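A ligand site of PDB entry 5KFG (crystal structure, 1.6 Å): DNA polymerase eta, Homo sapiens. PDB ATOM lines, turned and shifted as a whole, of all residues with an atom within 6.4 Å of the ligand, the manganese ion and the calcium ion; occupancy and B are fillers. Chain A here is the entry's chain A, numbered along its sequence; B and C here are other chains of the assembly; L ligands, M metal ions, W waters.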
ATOM      1  N   ASP A  16     -27.398  11.806 -32.169  1.00  0.00           N
ATOM      2  CA  ASP A  16     -27.173  10.957 -31.006  1.00  0.00           C
ATOM      3  C   ASP A  16     -27.557  11.707 -29.731  1.00  0.00           C
ATOM      4  O   ASP A  16     -27.026  12.779 -29.475  1.00  0.00           O
ATOM      5  CB  ASP A  16     -25.695  10.554 -30.961  1.00  0.00           C
ATOM      6  CG  ASP A  16     -25.458   9.271 -30.191  1.00  0.00           C
ATOM      7  OD1 ASP A  16     -25.726   9.257 -28.979  1.00  0.00           O
ATOM      8  OD2 ASP A  16     -24.981   8.286 -30.801  1.00  0.00           O
ATOM      9  N   MET A  17     -28.451  11.149 -28.919  1.00  0.00           N
ATOM     10  CA  MET A  17     -28.899  11.891 -27.740  1.00  0.00           C
ATOM     11  C   MET A  17     -27.782  12.015 -26.696  1.00  0.00           C
ATOM     12  O   MET A  17     -26.998  11.098 -26.546  1.00  0.00           O
ATOM     13  CB  MET A  17     -30.120  11.219 -27.120  1.00  0.00           C
ATOM     14  CG  MET A  17     -31.245  10.949 -28.092  1.00  0.00           C
ATOM     15  SD  MET A  17     -31.810  12.413 -28.969  1.00  0.00           S
ATOM     16  CE  MET A  17     -32.380  13.404 -27.638  1.00  0.00           C
ATOM     17  N   ASP A  18     -27.707  13.141 -26.000  1.00  0.00           N
ATOM     18  CA  ASP A  18     -26.703  13.288 -24.939  1.00  0.00           C
ATOM     19  C   ASP A  18     -27.116  12.524 -23.685  1.00  0.00           C
ATOM     20  O   ASP A  18     -28.266  12.679 -23.235  1.00  0.00           O
ATOM     21  CB  ASP A  18     -26.515  14.750 -24.532  1.00  0.00           C
ATOM     22  CG  ASP A  18     -26.036  15.630 -25.677  1.00  0.00           C
ATOM     23  OD1 ASP A  18     -25.347  15.118 -26.580  1.00  0.00           O
ATOM     24  OD2 ASP A  18     -26.331  16.839 -25.647  1.00  0.00           O
ATOM     25  N   CYS A  19     -26.196  11.717 -23.156  1.00  0.00           N
ATOM     26  CA  CYS A  19     -26.398  10.920 -21.924  1.00  0.00           C
ATOM     27  C   CYS A  19     -27.863  10.502 -21.779  1.00  0.00           C
ATOM     28  O   CYS A  19     -28.556  10.911 -20.839  1.00  0.00           O
ATOM     29  CB  CYS A  19     -25.904  11.643 -20.665  1.00  0.00           C
ATOM     30  SG  CYS A  19     -26.476  13.328 -20.366  1.00  0.00           S
ATOM     31  N   PHE A  20     -28.341   9.711 -22.732  1.00  0.00           N
ATOM     32  CA  PHE A  20     -29.781   9.622 -23.008  1.00  0.00           C
ATOM     33  C   PHE A  20     -30.624   9.174 -21.811  1.00  0.00           C
ATOM     34  O   PHE A  20     -31.567   9.882 -21.447  1.00  0.00           O
ATOM     35  CB  PHE A  20     -30.043   8.675 -24.192  1.00  0.00           C
ATOM     36  CG  PHE A  20     -31.492   8.593 -24.587  1.00  0.00           C
ATOM     37  CD1 PHE A  20     -32.256   9.736 -24.752  1.00  0.00           C
ATOM     38  CD2 PHE A  20     -32.103   7.361 -24.776  1.00  0.00           C
ATOM     39  CE1 PHE A  20     -33.603   9.656 -25.111  1.00  0.00           C
ATOM     40  CE2 PHE A  20     -33.451   7.277 -25.149  1.00  0.00           C
ATOM     41  CZ  PHE A  20     -34.187   8.420 -25.317  1.00  0.00           C
ATOM     42  N   PHE A  21     -30.299   8.041 -21.180  1.00  0.00           N
ATOM     43  CA  PHE A  21     -31.165   7.582 -20.096  1.00  0.00           C
ATOM     44  C   PHE A  21     -31.168   8.595 -18.948  1.00  0.00           C
ATOM     45  O   PHE A  21     -32.171   8.740 -18.255  1.00  0.00           O
ATOM     46  CB  PHE A  21     -30.762   6.207 -19.549  1.00  0.00           C
ATOM     47  CG  PHE A  21     -31.017   5.056 -20.467  1.00  0.00           C
ATOM     48  CD1 PHE A  21     -31.341   5.218 -21.809  1.00  0.00           C
ATOM     49  CD2 PHE A  21     -30.923   3.764 -19.972  1.00  0.00           C
ATOM     50  CE1 PHE A  21     -31.568   4.105 -22.631  1.00  0.00           C
ATOM     51  CE2 PHE A  21     -31.156   2.653 -20.786  1.00  0.00           C
ATOM     52  CZ  PHE A  21     -31.457   2.830 -22.112  1.00  0.00           C
ATOM     53  N   VAL A  22     -30.045   9.266 -18.725  1.00  0.00           N
ATOM     54  CA  VAL A  22     -30.001  10.315 -17.709  1.00  0.00           C
ATOM     55  C   VAL A  22     -30.963  11.456 -18.050  1.00  0.00           C
ATOM     56  O   VAL A  22     -31.705  11.935 -17.186  1.00  0.00           O
ATOM     57  CB  VAL A  22     -28.562  10.853 -17.540  1.00  0.00           C
ATOM     58  CG1 VAL A  22     -28.556  12.213 -16.816  1.00  0.00           C
ATOM     59  CG2 VAL A  22     -27.690   9.814 -16.801  1.00  0.00           C
ATOM     60  N   GLN A  41     -28.805   0.058 -12.774  1.00  0.00           N
ATOM     61  CA  GLN A  41     -29.758  -1.049 -12.715  1.00  0.00           C
ATOM     62  C   GLN A  41     -29.355  -2.008 -11.623  1.00  0.00           C
ATOM     63  O   GLN A  41     -28.184  -2.312 -11.428  1.00  0.00           O
ATOM     64  CB  GLN A  41     -29.934  -1.749 -14.065  1.00  0.00           C
ATOM     65  CG  GLN A  41     -28.703  -2.259 -14.744  1.00  0.00           C
ATOM     66  CD  GLN A  41     -28.958  -2.660 -16.203  1.00  0.00           C
ATOM     67  OE1 GLN A  41     -30.057  -2.476 -16.753  1.00  0.00           O
ATOM     68  NE2 GLN A  41     -27.936  -3.200 -16.828  1.00  0.00           N
ATOM     69  N   ILE A  51     -25.287   2.556 -16.065  1.00  0.00           N
ATOM     70  CA  ILE A  51     -25.412   2.414 -17.504  1.00  0.00           C
ATOM     71  C   ILE A  51     -25.484   3.749 -18.250  1.00  0.00           C
ATOM     72  O   ILE A  51     -25.401   3.759 -19.462  1.00  0.00           O
ATOM     73  CB  ILE A  51     -26.628   1.545 -17.906  1.00  0.00           C
ATOM     74  CG1 ILE A  51     -27.959   2.123 -17.415  1.00  0.00           C
ATOM     75  CG2 ILE A  51     -26.428   0.095 -17.425  1.00  0.00           C
ATOM     76  CD1 ILE A  51     -29.186   1.358 -17.964  1.00  0.00           C
ATOM     77  N   ALA A  52     -25.612   4.858 -17.525  1.00  0.00           N
ATOM     78  CA  ALA A  52     -25.590   6.186 -18.159  1.00  0.00           C
ATOM     79  C   ALA A  52     -25.149   7.224 -17.141  1.00  0.00           C
ATOM     80  O   ALA A  52     -25.448   7.075 -15.961  1.00  0.00           O
ATOM     81  CB  ALA A  52     -26.969   6.550 -18.746  1.00  0.00           C
ATOM     82  N   VAL A  53     -24.410   8.247 -17.587  1.00  0.00           N
ATOM     83  CA  VAL A  53     -23.753   9.211 -16.697  1.00  0.00           C
ATOM     84  C   VAL A  53     -23.871  10.630 -17.220  1.00  0.00           C
ATOM     85  O   VAL A  53     -23.515  10.887 -18.391  1.00  0.00           O
ATOM     86  CB  VAL A  53     -22.245   8.890 -16.553  1.00  0.00           C
ATOM     87  CG1 VAL A  53     -21.582   9.767 -15.498  1.00  0.00           C
ATOM     88  CG2 VAL A  53     -22.021   7.419 -16.222  1.00  0.00           C
ATOM     89  N   TYR A  55     -22.934  14.603 -17.768  1.00  0.00           N
ATOM     90  CA  TYR A  55     -21.634  15.203 -18.026  1.00  0.00           C
ATOM     91  C   TYR A  55     -21.033  15.814 -16.765  1.00  0.00           C
ATOM     92  O   TYR A  55     -19.815  15.784 -16.600  1.00  0.00           O
ATOM     93  CB  TYR A  55     -21.743  16.229 -19.160  1.00  0.00           C
ATOM     94  CG  TYR A  55     -21.761  15.508 -20.486  1.00  0.00           C
ATOM     95  CD1 TYR A  55     -22.933  14.929 -20.967  1.00  0.00           C
ATOM     96  CD2 TYR A  55     -20.606  15.332 -21.226  1.00  0.00           C
ATOM     97  CE1 TYR A  55     -22.954  14.218 -22.148  1.00  0.00           C
ATOM     98  CE2 TYR A  55     -20.614  14.627 -22.424  1.00  0.00           C
ATOM     99  CZ  TYR A  55     -21.784  14.075 -22.884  1.00  0.00           C
ATOM    100  OH  TYR A  55     -21.784  13.362 -24.073  1.00  0.00           O
ATOM    101  N   ARG A  58     -19.376  12.868 -15.149  1.00  0.00           N
ATOM    102  CA  ARG A  58     -18.192  12.414 -15.885  1.00  0.00           C
ATOM    103  C   ARG A  58     -16.955  13.214 -15.473  1.00  0.00           C
ATOM    104  O   ARG A  58     -15.837  12.686 -15.512  1.00  0.00           O
ATOM    105  CB  ARG A  58     -18.408  12.545 -17.381  1.00  0.00           C
ATOM    106  CG  ARG A  58     -19.511  11.679 -17.889  1.00  0.00           C
ATOM    107  CD  ARG A  58     -19.662  11.802 -19.380  1.00  0.00           C
ATOM    108  NE  ARG A  58     -20.963  11.255 -19.779  1.00  0.00           N
ATOM    109  CZ  ARG A  58     -21.342  10.978 -21.012  1.00  0.00           C
ATOM    110  NH1 ARG A  58     -20.499  11.154 -22.028  1.00  0.00           N
ATOM    111  NH2 ARG A  58     -22.565  10.483 -21.233  1.00  0.00           N
ATOM    112  N   ARG A  64     -19.734   4.547 -17.354  1.00  0.00           N
ATOM    113  CA  ARG A  64     -20.515   3.362 -17.544  1.00  0.00           C
ATOM    114  C   ARG A  64     -19.759   2.115 -17.127  1.00  0.00           C
ATOM    115  O   ARG A  64     -18.574   2.066 -17.205  1.00  0.00           O
ATOM    116  CB  ARG A  64     -20.970   3.295 -19.023  1.00  0.00           C
ATOM    117  CG  ARG A  64     -21.680   2.064 -19.493  1.00  0.00           C
ATOM    118  CD  ARG A  64     -21.993   2.241 -20.965  1.00  0.00           C
ATOM    119  NE  ARG A  64     -23.024   3.222 -21.093  1.00  0.00           N
ATOM    120  CZ  ARG A  64     -23.085   4.205 -21.982  1.00  0.00           C
ATOM    121  NH1 ARG A  64     -22.212   4.356 -22.978  1.00  0.00           N
ATOM    122  NH2 ARG A  64     -24.119   4.985 -21.867  1.00  0.00           N
ATOM    123  N   LEU A  92     -36.784  -1.810 -19.631  1.00  0.00           N
ATOM    124  CA  LEU A  92     -36.295  -0.582 -20.286  1.00  0.00           C
ATOM    125  C   LEU A  92     -37.390   0.174 -21.052  1.00  0.00           C
ATOM    126  O   LEU A  92     -37.085   1.026 -21.881  1.00  0.00           O
ATOM    127  CB  LEU A  92     -35.148  -0.918 -21.223  1.00  0.00           C
ATOM    128  CG  LEU A  92     -34.015  -1.744 -20.595  1.00  0.00           C
ATOM    129  CD1 LEU A  92     -33.019  -2.160 -21.659  1.00  0.00           C
ATOM    130  CD2 LEU A  92     -33.341  -0.909 -19.507  1.00  0.00           C
ATOM    131  N   SER A 116     -29.656   2.747 -32.908  1.00  0.00           N
ATOM    132  CA  SER A 116     -29.648   2.322 -31.518  1.00  0.00           C
ATOM    133  C   SER A 116     -30.842   2.941 -30.821  1.00  0.00           C
ATOM    134  O   SER A 116     -31.606   3.675 -31.437  1.00  0.00           O
ATOM    135  CB  SER A 116     -28.365   2.741 -30.801  1.00  0.00           C
ATOM    136  OG  SER A 116     -28.451   4.082 -30.360  1.00  0.00           O
ATOM    137  N   ILE A 117     -30.982   2.683 -29.527  1.00  0.00           N
ATOM    138  CA  ILE A 117     -32.081   3.255 -28.787  1.00  0.00           C
ATOM    139  C   ILE A 117     -32.003   4.796 -28.785  1.00  0.00           C
ATOM    140  O   ILE A 117     -33.025   5.457 -28.614  1.00  0.00           O
ATOM    141  CB  ILE A 117     -32.124   2.703 -27.327  1.00  0.00           C
ATOM    142  CG1 ILE A 117     -33.500   2.947 -26.693  1.00  0.00           C
ATOM    143  CG2 ILE A 117     -30.982   3.307 -26.497  1.00  0.00           C
ATOM    144  CD1 ILE A 117     -33.712   2.169 -25.391  1.00  0.00           C
ATOM    145  N   ASP A 118     -30.819   5.371 -28.975  1.00  0.00           N
ATOM    146  CA  ASP A 118     -30.746   6.830 -28.860  1.00  0.00           C
ATOM    147  C   ASP A 118     -30.094   7.512 -30.058  1.00  0.00           C
ATOM    148  O   ASP A 118     -29.681   8.673 -29.958  1.00  0.00           O
ATOM    149  CB  ASP A 118     -30.015   7.223 -27.576  1.00  0.00           C
ATOM    150  CG  ASP A 118     -28.503   7.290 -27.750  1.00  0.00           C
ATOM    151  OD1 ASP A 118     -27.921   6.433 -28.464  1.00  0.00           O
ATOM    152  OD2 ASP A 118     -27.907   8.249 -27.200  1.00  0.00           O
ATOM    153  N   GLU A 119     -30.004   6.828 -31.189  1.00  0.00           N
ATOM    154  CA  GLU A 119     -29.442   7.506 -32.356  1.00  0.00           C
ATOM    155  C   GLU A 119     -29.956   6.994 -33.675  1.00  0.00           C
ATOM    156  O   GLU A 119     -30.391   5.847 -33.799  1.00  0.00           O
ATOM    157  CB  GLU A 119     -27.937   7.418 -32.344  1.00  0.00           C
ATOM    158  CG  GLU A 119     -27.383   6.088 -32.781  1.00  0.00           C
ATOM    159  CD  GLU A 119     -26.056   5.815 -32.127  1.00  0.00           C
ATOM    160  OE1 GLU A 119     -25.008   5.948 -32.799  1.00  0.00           O
ATOM    161  OE2 GLU A 119     -26.047   5.495 -30.915  1.00  0.00           O
ATOM    162  N   SER A 216     -26.413  15.621 -29.806  1.00  0.00           N
ATOM    163  CA  SER A 216     -25.316  16.036 -30.659  1.00  0.00           C
ATOM    164  C   SER A 216     -25.522  15.442 -32.036  1.00  0.00           C
ATOM    165  O   SER A 216     -26.350  14.556 -32.197  1.00  0.00           O
ATOM    166  CB  SER A 216     -23.986  15.589 -30.066  1.00  0.00           C
ATOM    167  OG  SER A 216     -23.810  16.213 -28.805  1.00  0.00           O
ATOM    168  N   LYS A 227     -20.911   9.592 -37.953  1.00  0.00           N
ATOM    169  CA  LYS A 227     -20.829   9.163 -36.619  1.00  0.00           C
ATOM    170  C   LYS A 227     -19.552   9.636 -35.895  1.00  0.00           C
ATOM    171  O   LYS A 227     -19.563   9.992 -34.757  1.00  0.00           O
ATOM    172  CB  LYS A 227     -20.812   7.589 -36.487  1.00  0.00           C
ATOM    173  CG  LYS A 227     -20.580   6.857 -35.240  1.00  0.00           C
ATOM    174  CD  LYS A 227     -21.682   7.237 -34.261  1.00  0.00           C
ATOM    175  CE  LYS A 227     -21.484   6.537 -32.902  1.00  0.00           C
ATOM    176  NZ  LYS A 227     -22.556   6.849 -31.905  1.00  0.00           N
ATOM    177  N   LYS A 234     -19.385  16.781 -28.537  1.00  0.00           N
ATOM    178  CA  LYS A 234     -20.488  16.582 -27.582  1.00  0.00           C
ATOM    179  C   LYS A 234     -20.178  17.232 -26.237  1.00  0.00           C
ATOM    180  O   LYS A 234     -19.053  17.373 -25.900  1.00  0.00           O
ATOM    181  CB  LYS A 234     -20.779  15.085 -27.485  1.00  0.00           C
ATOM    182  CG  LYS A 234     -19.681  14.318 -26.864  1.00  0.00           C
ATOM    183  CD  LYS A 234     -19.902  12.819 -26.963  1.00  0.00           C
ATOM    184  CE  LYS A 234     -19.242  12.133 -25.770  1.00  0.00           C
ATOM    185  NZ  LYS A 234     -19.521  10.665 -25.792  1.00  0.00           N
ATOM    186  N   PRO A 235     -21.171  17.625 -25.328  1.00  0.00           N
ATOM    187  CA  PRO A 235     -22.565  17.468 -25.736  1.00  0.00           C
ATOM    188  C   PRO A 235     -23.241  18.700 -26.324  1.00  0.00           C
ATOM    189  O   PRO A 235     -22.672  19.716 -26.305  1.00  0.00           O
ATOM    190  CB  PRO A 235     -23.249  17.166 -24.408  1.00  0.00           C
ATOM    191  CG  PRO A 235     -22.614  18.046 -23.448  1.00  0.00           C
ATOM    192  CD  PRO A 235     -21.205  18.060 -23.835  1.00  0.00           C
ATOM    193  P    DT B   8     -20.874   2.299 -30.046  1.00  0.00           P
ATOM    194  OP1  DT B   8     -20.686   3.666 -30.555  1.00  0.00           O
ATOM    195  OP2  DT B   8     -20.055   1.798 -28.911  1.00  0.00           O
ATOM    196  O5'  DT B   8     -22.429   2.096 -29.616  1.00  0.00           O
ATOM    197  C5'  DT B   8     -23.583   2.594 -30.407  1.00  0.00           C
ATOM    198  C4'  DT B   8     -24.818   2.531 -29.511  1.00  0.00           C
ATOM    199  O4'  DT B   8     -24.852   1.170 -29.030  1.00  0.00           O
ATOM    200  C3'  DT B   8     -24.626   3.439 -28.311  1.00  0.00           C
ATOM    201  O3'  DT B   8     -25.760   4.246 -28.130  1.00  0.00           O
ATOM    202  C2'  DT B   8     -24.414   2.470 -27.128  1.00  0.00           C
ATOM    203  C1'  DT B   8     -25.042   1.180 -27.631  1.00  0.00           C
ATOM    204  N1   DT B   8     -24.393  -0.020 -27.035  1.00  0.00           N
ATOM    205  C2   DT B   8     -25.139  -0.859 -26.236  1.00  0.00           C
ATOM    206  O2   DT B   8     -26.319  -0.690 -25.993  1.00  0.00           O
ATOM    207  N3   DT B   8     -24.440  -1.912 -25.715  1.00  0.00           N
ATOM    208  C4   DT B   8     -23.107  -2.209 -25.910  1.00  0.00           C
ATOM    209  O4   DT B   8     -22.572  -3.187 -25.406  1.00  0.00           O
ATOM    210  C5   DT B   8     -22.392  -1.278 -26.749  1.00  0.00           C
ATOM    211  C7   DT B   8     -20.931  -1.502 -27.027  1.00  0.00           C
ATOM    212  C6   DT B   8     -23.056  -0.242 -27.260  1.00  0.00           C
ATOM    213  P    DT C   3     -17.746  -8.053 -13.181  1.00  0.00           P
ATOM    214  OP1  DT C   3     -17.146  -9.229 -13.849  1.00  0.00           O
ATOM    215  OP2  DT C   3     -16.939  -7.197 -12.279  1.00  0.00           O
ATOM    216  O5'  DT C   3     -18.393  -7.119 -14.306  1.00  0.00           O
ATOM    217  C5'  DT C   3     -19.323  -6.123 -13.951  1.00  0.00           C
ATOM    218  C4'  DT C   3     -20.105  -5.674 -15.162  1.00  0.00           C
ATOM    219  O4'  DT C   3     -19.313  -4.753 -15.931  1.00  0.00           O
ATOM    220  C3'  DT C   3     -20.484  -6.816 -16.111  1.00  0.00           C
ATOM    221  O3'  DT C   3     -21.901  -6.865 -16.282  1.00  0.00           O
ATOM    222  C2'  DT C   3     -19.748  -6.485 -17.414  1.00  0.00           C
ATOM    223  C1'  DT C   3     -19.512  -4.991 -17.300  1.00  0.00           C
ATOM    224  N1   DT C   3     -18.312  -4.516 -18.023  1.00  0.00           N
ATOM    225  C2   DT C   3     -18.449  -3.529 -18.967  1.00  0.00           C
ATOM    226  O2   DT C   3     -19.521  -3.020 -19.251  1.00  0.00           O
ATOM    227  N3   DT C   3     -17.284  -3.169 -19.581  1.00  0.00           N
ATOM    228  C4   DT C   3     -16.025  -3.678 -19.348  1.00  0.00           C
ATOM    229  O4   DT C   3     -15.022  -3.278 -19.954  1.00  0.00           O
ATOM    230  C5   DT C   3     -15.947  -4.713 -18.349  1.00  0.00           C
ATOM    231  C7   DT C   3     -14.630  -5.345 -18.005  1.00  0.00           C
ATOM    232  C6   DT C   3     -17.084  -5.073 -17.738  1.00  0.00           C
ATOM    233  P    DT C   4     -22.701  -8.170 -15.802  1.00  0.00           P
ATOM    234  OP1  DT C   4     -22.419  -8.378 -14.363  1.00  0.00           O
ATOM    235  OP2  DT C   4     -22.373  -9.224 -16.787  1.00  0.00           O
ATOM    236  O5'  DT C   4     -24.244  -7.801 -16.032  1.00  0.00           O
ATOM    237  C5'  DT C   4     -25.050  -7.212 -14.995  1.00  0.00           C
ATOM    238  C4'  DT C   4     -26.338  -6.655 -15.607  1.00  0.00           C
ATOM    239  O4'  DT C   4     -25.964  -5.615 -16.547  1.00  0.00           O
ATOM    240  C3'  DT C   4     -27.139  -7.673 -16.419  1.00  0.00           C
ATOM    241  O3'  DT C   4     -28.514  -7.340 -16.312  1.00  0.00           O
ATOM    242  C2'  DT C   4     -26.604  -7.473 -17.838  1.00  0.00           C
ATOM    243  C1'  DT C   4     -26.405  -5.963 -17.844  1.00  0.00           C
ATOM    244  N1   DT C   4     -25.401  -5.442 -18.794  1.00  0.00           N
ATOM    245  C2   DT C   4     -25.673  -4.252 -19.380  1.00  0.00           C
ATOM    246  O2   DT C   4     -26.723  -3.653 -19.204  1.00  0.00           O
ATOM    247  N3   DT C   4     -24.709  -3.783 -20.216  1.00  0.00           N
ATOM    248  C4   DT C   4     -23.505  -4.359 -20.505  1.00  0.00           C
ATOM    249  O4   DT C   4     -22.699  -3.843 -21.276  1.00  0.00           O
ATOM    250  C5   DT C   4     -23.255  -5.620 -19.839  1.00  0.00           C
ATOM    251  C7   DT C   4     -21.968  -6.367 -20.079  1.00  0.00           C
ATOM    252  C6   DT C   4     -24.204  -6.089 -19.004  1.00  0.00           C
ATOM    253  P    DA C   5     -29.640  -8.233 -17.023  1.00  0.00           P
ATOM    254  OP1  DA C   5     -30.773  -8.304 -16.089  1.00  0.00           O
ATOM    255  OP2  DA C   5     -29.023  -9.466 -17.566  1.00  0.00           O
ATOM    256  O5'  DA C   5     -30.056  -7.353 -18.283  1.00  0.00           O
ATOM    257  C5'  DA C   5     -30.700  -6.094 -18.085  1.00  0.00           C
ATOM    258  C4'  DA C   5     -31.080  -5.493 -19.416  1.00  0.00           C
ATOM    259  O4'  DA C   5     -29.879  -5.043 -20.117  1.00  0.00           O
ATOM    260  C3'  DA C   5     -31.764  -6.456 -20.370  1.00  0.00           C
ATOM    261  O3'  DA C   5     -32.757  -5.750 -21.100  1.00  0.00           O
ATOM    262  C2'  DA C   5     -30.629  -6.921 -21.284  1.00  0.00           C
ATOM    263  C1'  DA C   5     -29.859  -5.609 -21.410  1.00  0.00           C
ATOM    264  N9   DA C   5     -28.473  -5.769 -21.825  1.00  0.00           N
ATOM    265  C8   DA C   5     -27.616  -6.765 -21.481  1.00  0.00           C
ATOM    266  N7   DA C   5     -26.415  -6.624 -21.991  1.00  0.00           N
ATOM    267  C5   DA C   5     -26.491  -5.435 -22.702  1.00  0.00           C
ATOM    268  C6   DA C   5     -25.551  -4.733 -23.485  1.00  0.00           C
ATOM    269  N6   DA C   5     -24.296  -5.151 -23.662  1.00  0.00           N
ATOM    270  N1   DA C   5     -25.950  -3.585 -24.063  1.00  0.00           N
ATOM    271  C2   DA C   5     -27.219  -3.173 -23.869  1.00  0.00           C
ATOM    272  N3   DA C   5     -28.193  -3.752 -23.163  1.00  0.00           N
ATOM    273  C4   DA C   5     -27.753  -4.894 -22.604  1.00  0.00           C
HETATM  274  P1  LIG L   1     -23.242  10.177 -24.663  1.00  0.00           P
HETATM  275  O1  LIG L   1     -23.714   9.652 -25.995  1.00  0.00           O
HETATM  276  O2  LIG L   1     -23.633  11.604 -24.407  1.00  0.00           O
HETATM  277  O3  LIG L   1     -21.733  10.006 -24.502  1.00  0.00           O
HETATM  278  P2  LIG L   1     -25.009   8.146 -23.663  1.00  0.00           P
HETATM  279  O4  LIG L   1     -26.165   8.665 -24.489  1.00  0.00           O
HETATM  280  O5  LIG L   1     -25.447   7.711 -22.273  1.00  0.00           O
HETATM  281  O6  LIG L   1     -23.896   9.303 -23.484  1.00  0.00           O
HETATM  282  P3  LIG L   1     -24.679   6.044 -25.624  1.00  0.00           P
HETATM  283  O7  LIG L   1     -25.048   6.882 -26.816  1.00  0.00           O
HETATM  284  O8  LIG L   1     -23.478   5.141 -25.857  1.00  0.00           O
HETATM  285  O9  LIG L   1     -24.247   6.935 -24.356  1.00  0.00           O
HETATM  286  O10 LIG L   1     -25.862   5.114 -25.147  1.00  0.00           O
HETATM  287  C1  LIG L   1     -27.186   5.584 -25.113  1.00  0.00           C
HETATM  288  C2  LIG L   1     -27.949   4.904 -23.974  1.00  0.00           C
HETATM  289  O11 LIG L   1     -27.959   3.508 -24.200  1.00  0.00           O
HETATM  290  C3  LIG L   1     -27.324   5.148 -22.691  1.00  0.00           C
HETATM  291  O12 LIG L   1     -27.838   6.349 -22.088  1.00  0.00           O
HETATM  292  C4  LIG L   1     -27.668   3.951 -21.901  1.00  0.00           C
HETATM  293  C5  LIG L   1     -27.741   2.865 -22.933  1.00  0.00           C
HETATM  294  N1  LIG L   1     -26.541   2.089 -23.011  1.00  0.00           N
HETATM  295  C6  LIG L   1     -25.410   2.378 -23.690  1.00  0.00           C
HETATM  296  N2  LIG L   1     -24.495   1.429 -23.511  1.00  0.00           N
HETATM  297  C7  LIG L   1     -25.024   0.475 -22.732  1.00  0.00           C
HETATM  298  C8  LIG L   1     -24.573  -0.730 -22.215  1.00  0.00           C
HETATM  299  N3  LIG L   1     -23.263  -1.185 -22.526  1.00  0.00           N
HETATM  300  N4  LIG L   1     -25.377  -1.450 -21.430  1.00  0.00           N
HETATM  301  C9  LIG L   1     -26.637  -1.058 -21.127  1.00  0.00           C
HETATM  302  N5  LIG L   1     -27.114   0.126 -21.607  1.00  0.00           N
HETATM  303  C10 LIG L   1     -26.331   0.886 -22.394  1.00  0.00           C
HETATM  304 MN    MN M   1     -25.779   6.395 -29.017  1.00  0.00          MN
HETATM  305 CA    CA M   2     -25.881   9.174 -26.774  1.00  0.00          CA
HETATM  306  O   HOH W   1     -22.134   8.383 -27.650  1.00  0.00           O
HETATM  307  O   HOH W   2     -29.878  -0.309 -21.497  1.00  0.00           O
HETATM  308  O   HOH W   3     -23.631   6.512 -29.210  1.00  0.00           O
HETATM  309  O   HOH W   4     -28.597   0.347 -25.280  1.00  0.00           O
HETATM  310  O   HOH W   5     -21.760   1.066 -24.268  1.00  0.00           O
HETATM  311  O   HOH W   6     -27.673   2.894 -27.181  1.00  0.00           O
HETATM  312  O   HOH W   7     -20.597   7.813 -23.563  1.00  0.00           O
HETATM  313  O   HOH W   8     -23.733   7.972 -20.282  1.00  0.00           O
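O3 of the ligand is in salt-bridge range of NH1 of Arg 58, 3.0 Å away.
O12 of the ligand sits at hydrogen-bond distance from N of Phe 20, at 3.5 Å.
An oxygen (O2) of the ligand sits at hydrogen-bond distance from the backbone NH (N) of Cys 19.
OH of Tyr 55 sits at hydrogen-bond distance from O2 of the ligand, at 2.6 Å.
N of Phe 21 is in hydrogen-bond range of O12 of the ligand.
O4 of DT 4 of chain C sits at hydrogen-bond distance from N3 of the ligand (3.0 Å).
An oxygen (O5) of the ligand lies within salt-bridge range of the guanidinium group (NH2) of Arg 64.
N3 of DT 8 of chain B lies within hydrogen-bond range of a nitrogen (N3) of the ligand (3.5 Å).
NZ of Lys 234 is in salt-bridge range of O3 of the ligand.
O2 of DT 4 of chain C is in hydrogen-bond range of the side-chain amide nitrogen of Gln 41 (2.7 Å).
NZ of Lys 227 is in salt-bridge range of OE1 of Glu 119 (2.8 Å).
The guanidinium group (NE) of Arg 58 lies within hydrogen-bond range of the backbone carbonyl oxygen (O) of Val 53 (2.9 Å).
OD2 of Asp 16 is in salt-bridge range of NZ of Lys 227, 3.0 Å away.
N of Asp 118 lies within hydrogen-bond range of OG of Ser 116 (3.0 Å).
The side-chain hydroxyl (OH) of Tyr 55 sits at hydrogen-bond distance from the guanidinium group (NH1) of Arg 58 (3.3 Å).
The side-chain hydroxyl (OG) of Ser 216 lies within hydrogen-bond range of the side-chain carboxylate (OD1) of Asp 18, 2.9 Å away.
OP1 of DT 8 of chain B lies within salt-bridge range of NZ of Lys 227 (3.9 Å).
N1 of DA 5 of chain C sits close to N4 of the ligand (3.4 Å).
Asp 18 touches the ligand (CA to O2, 3.5 Å).
Ile 51 touches the ligand.
CB of Ala 52 touches O12 of the ligand, 3.5 Å away.
Ile 117 touches the ligand.
Hydrophobic or aromatic side chains that line the ligand: Phe 20, Phe 21, Ile 51, Ala 52, Tyr 55 and Ile 117.
Within 4 Å of the ligand: Asp 16, Met 17, Asp 18, Cys 19, Phe 20, Phe 21, Ile 51, Ala 52, Tyr 55, Arg 58, Arg 64, Ile 117, Asp 118, Lys 234, DT 8 of chain B, DT 4 of chain C and DA 5 of chain C.
Ser 116 touches the manganese ion.
Of the 27 residues printed, 5 come within 4 Å of the manganese ion.
The nearest printed residue that does not touch the manganese ion is Lys 227 (4.4 Å).
Of the 27 residues printed, 3 come within 4 Å of the calcium ion.
Along chain A the residues within 4 Å of the calcium ion span positions 16 to 118.
The side-chain carboxylate (OE2) of Glu 119 binds the manganese ion.
The manganese ion is bound by water W3 (2.2 Å).
The manganese ion is bound by OD1 of Asp 118 (2.2 Å).
O3' of DT 8 of chain B is bound to the manganese ion, 2.3 Å away.
O7 of the ligand is bound to the manganese ion (2.4 Å).
Slightly farther from the manganese ion lies OD2 of Asp 16 (2.7 Å).
Slightly farther from the manganese ion lies OD1 of Asp 16 (2.9 Å).
The calcium ion is bound by the side-chain carboxylate of Asp 16 (2.2 Å), the backbone carbonyl oxygen of Met 17 (2.2 Å), the side-chain carboxylate of Asp 118 (2.3 Å), an oxygen (O1) of the ligand (2.4 Å), an oxygen (O4) of the ligand (2.4 Å) and an oxygen (O7) of the ligand (2.4 Å).
The calcium ion has six donor atoms within binding distance.
Water W3 lies within hydrogen-bond range of the side-chain carboxylate (OD2) of Asp 16 and the side-chain amino group (NZ) of Lys 227.
Water W6 bridges an oxygen (O11) of the ligand and the side-chain hydroxyl (OG) of Ser 116.
Water W4 lies within hydrogen-bond range of O2 of DT 8 of chain B (2.6 Å) and an oxygen (O11) of the ligand (3.4 Å).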
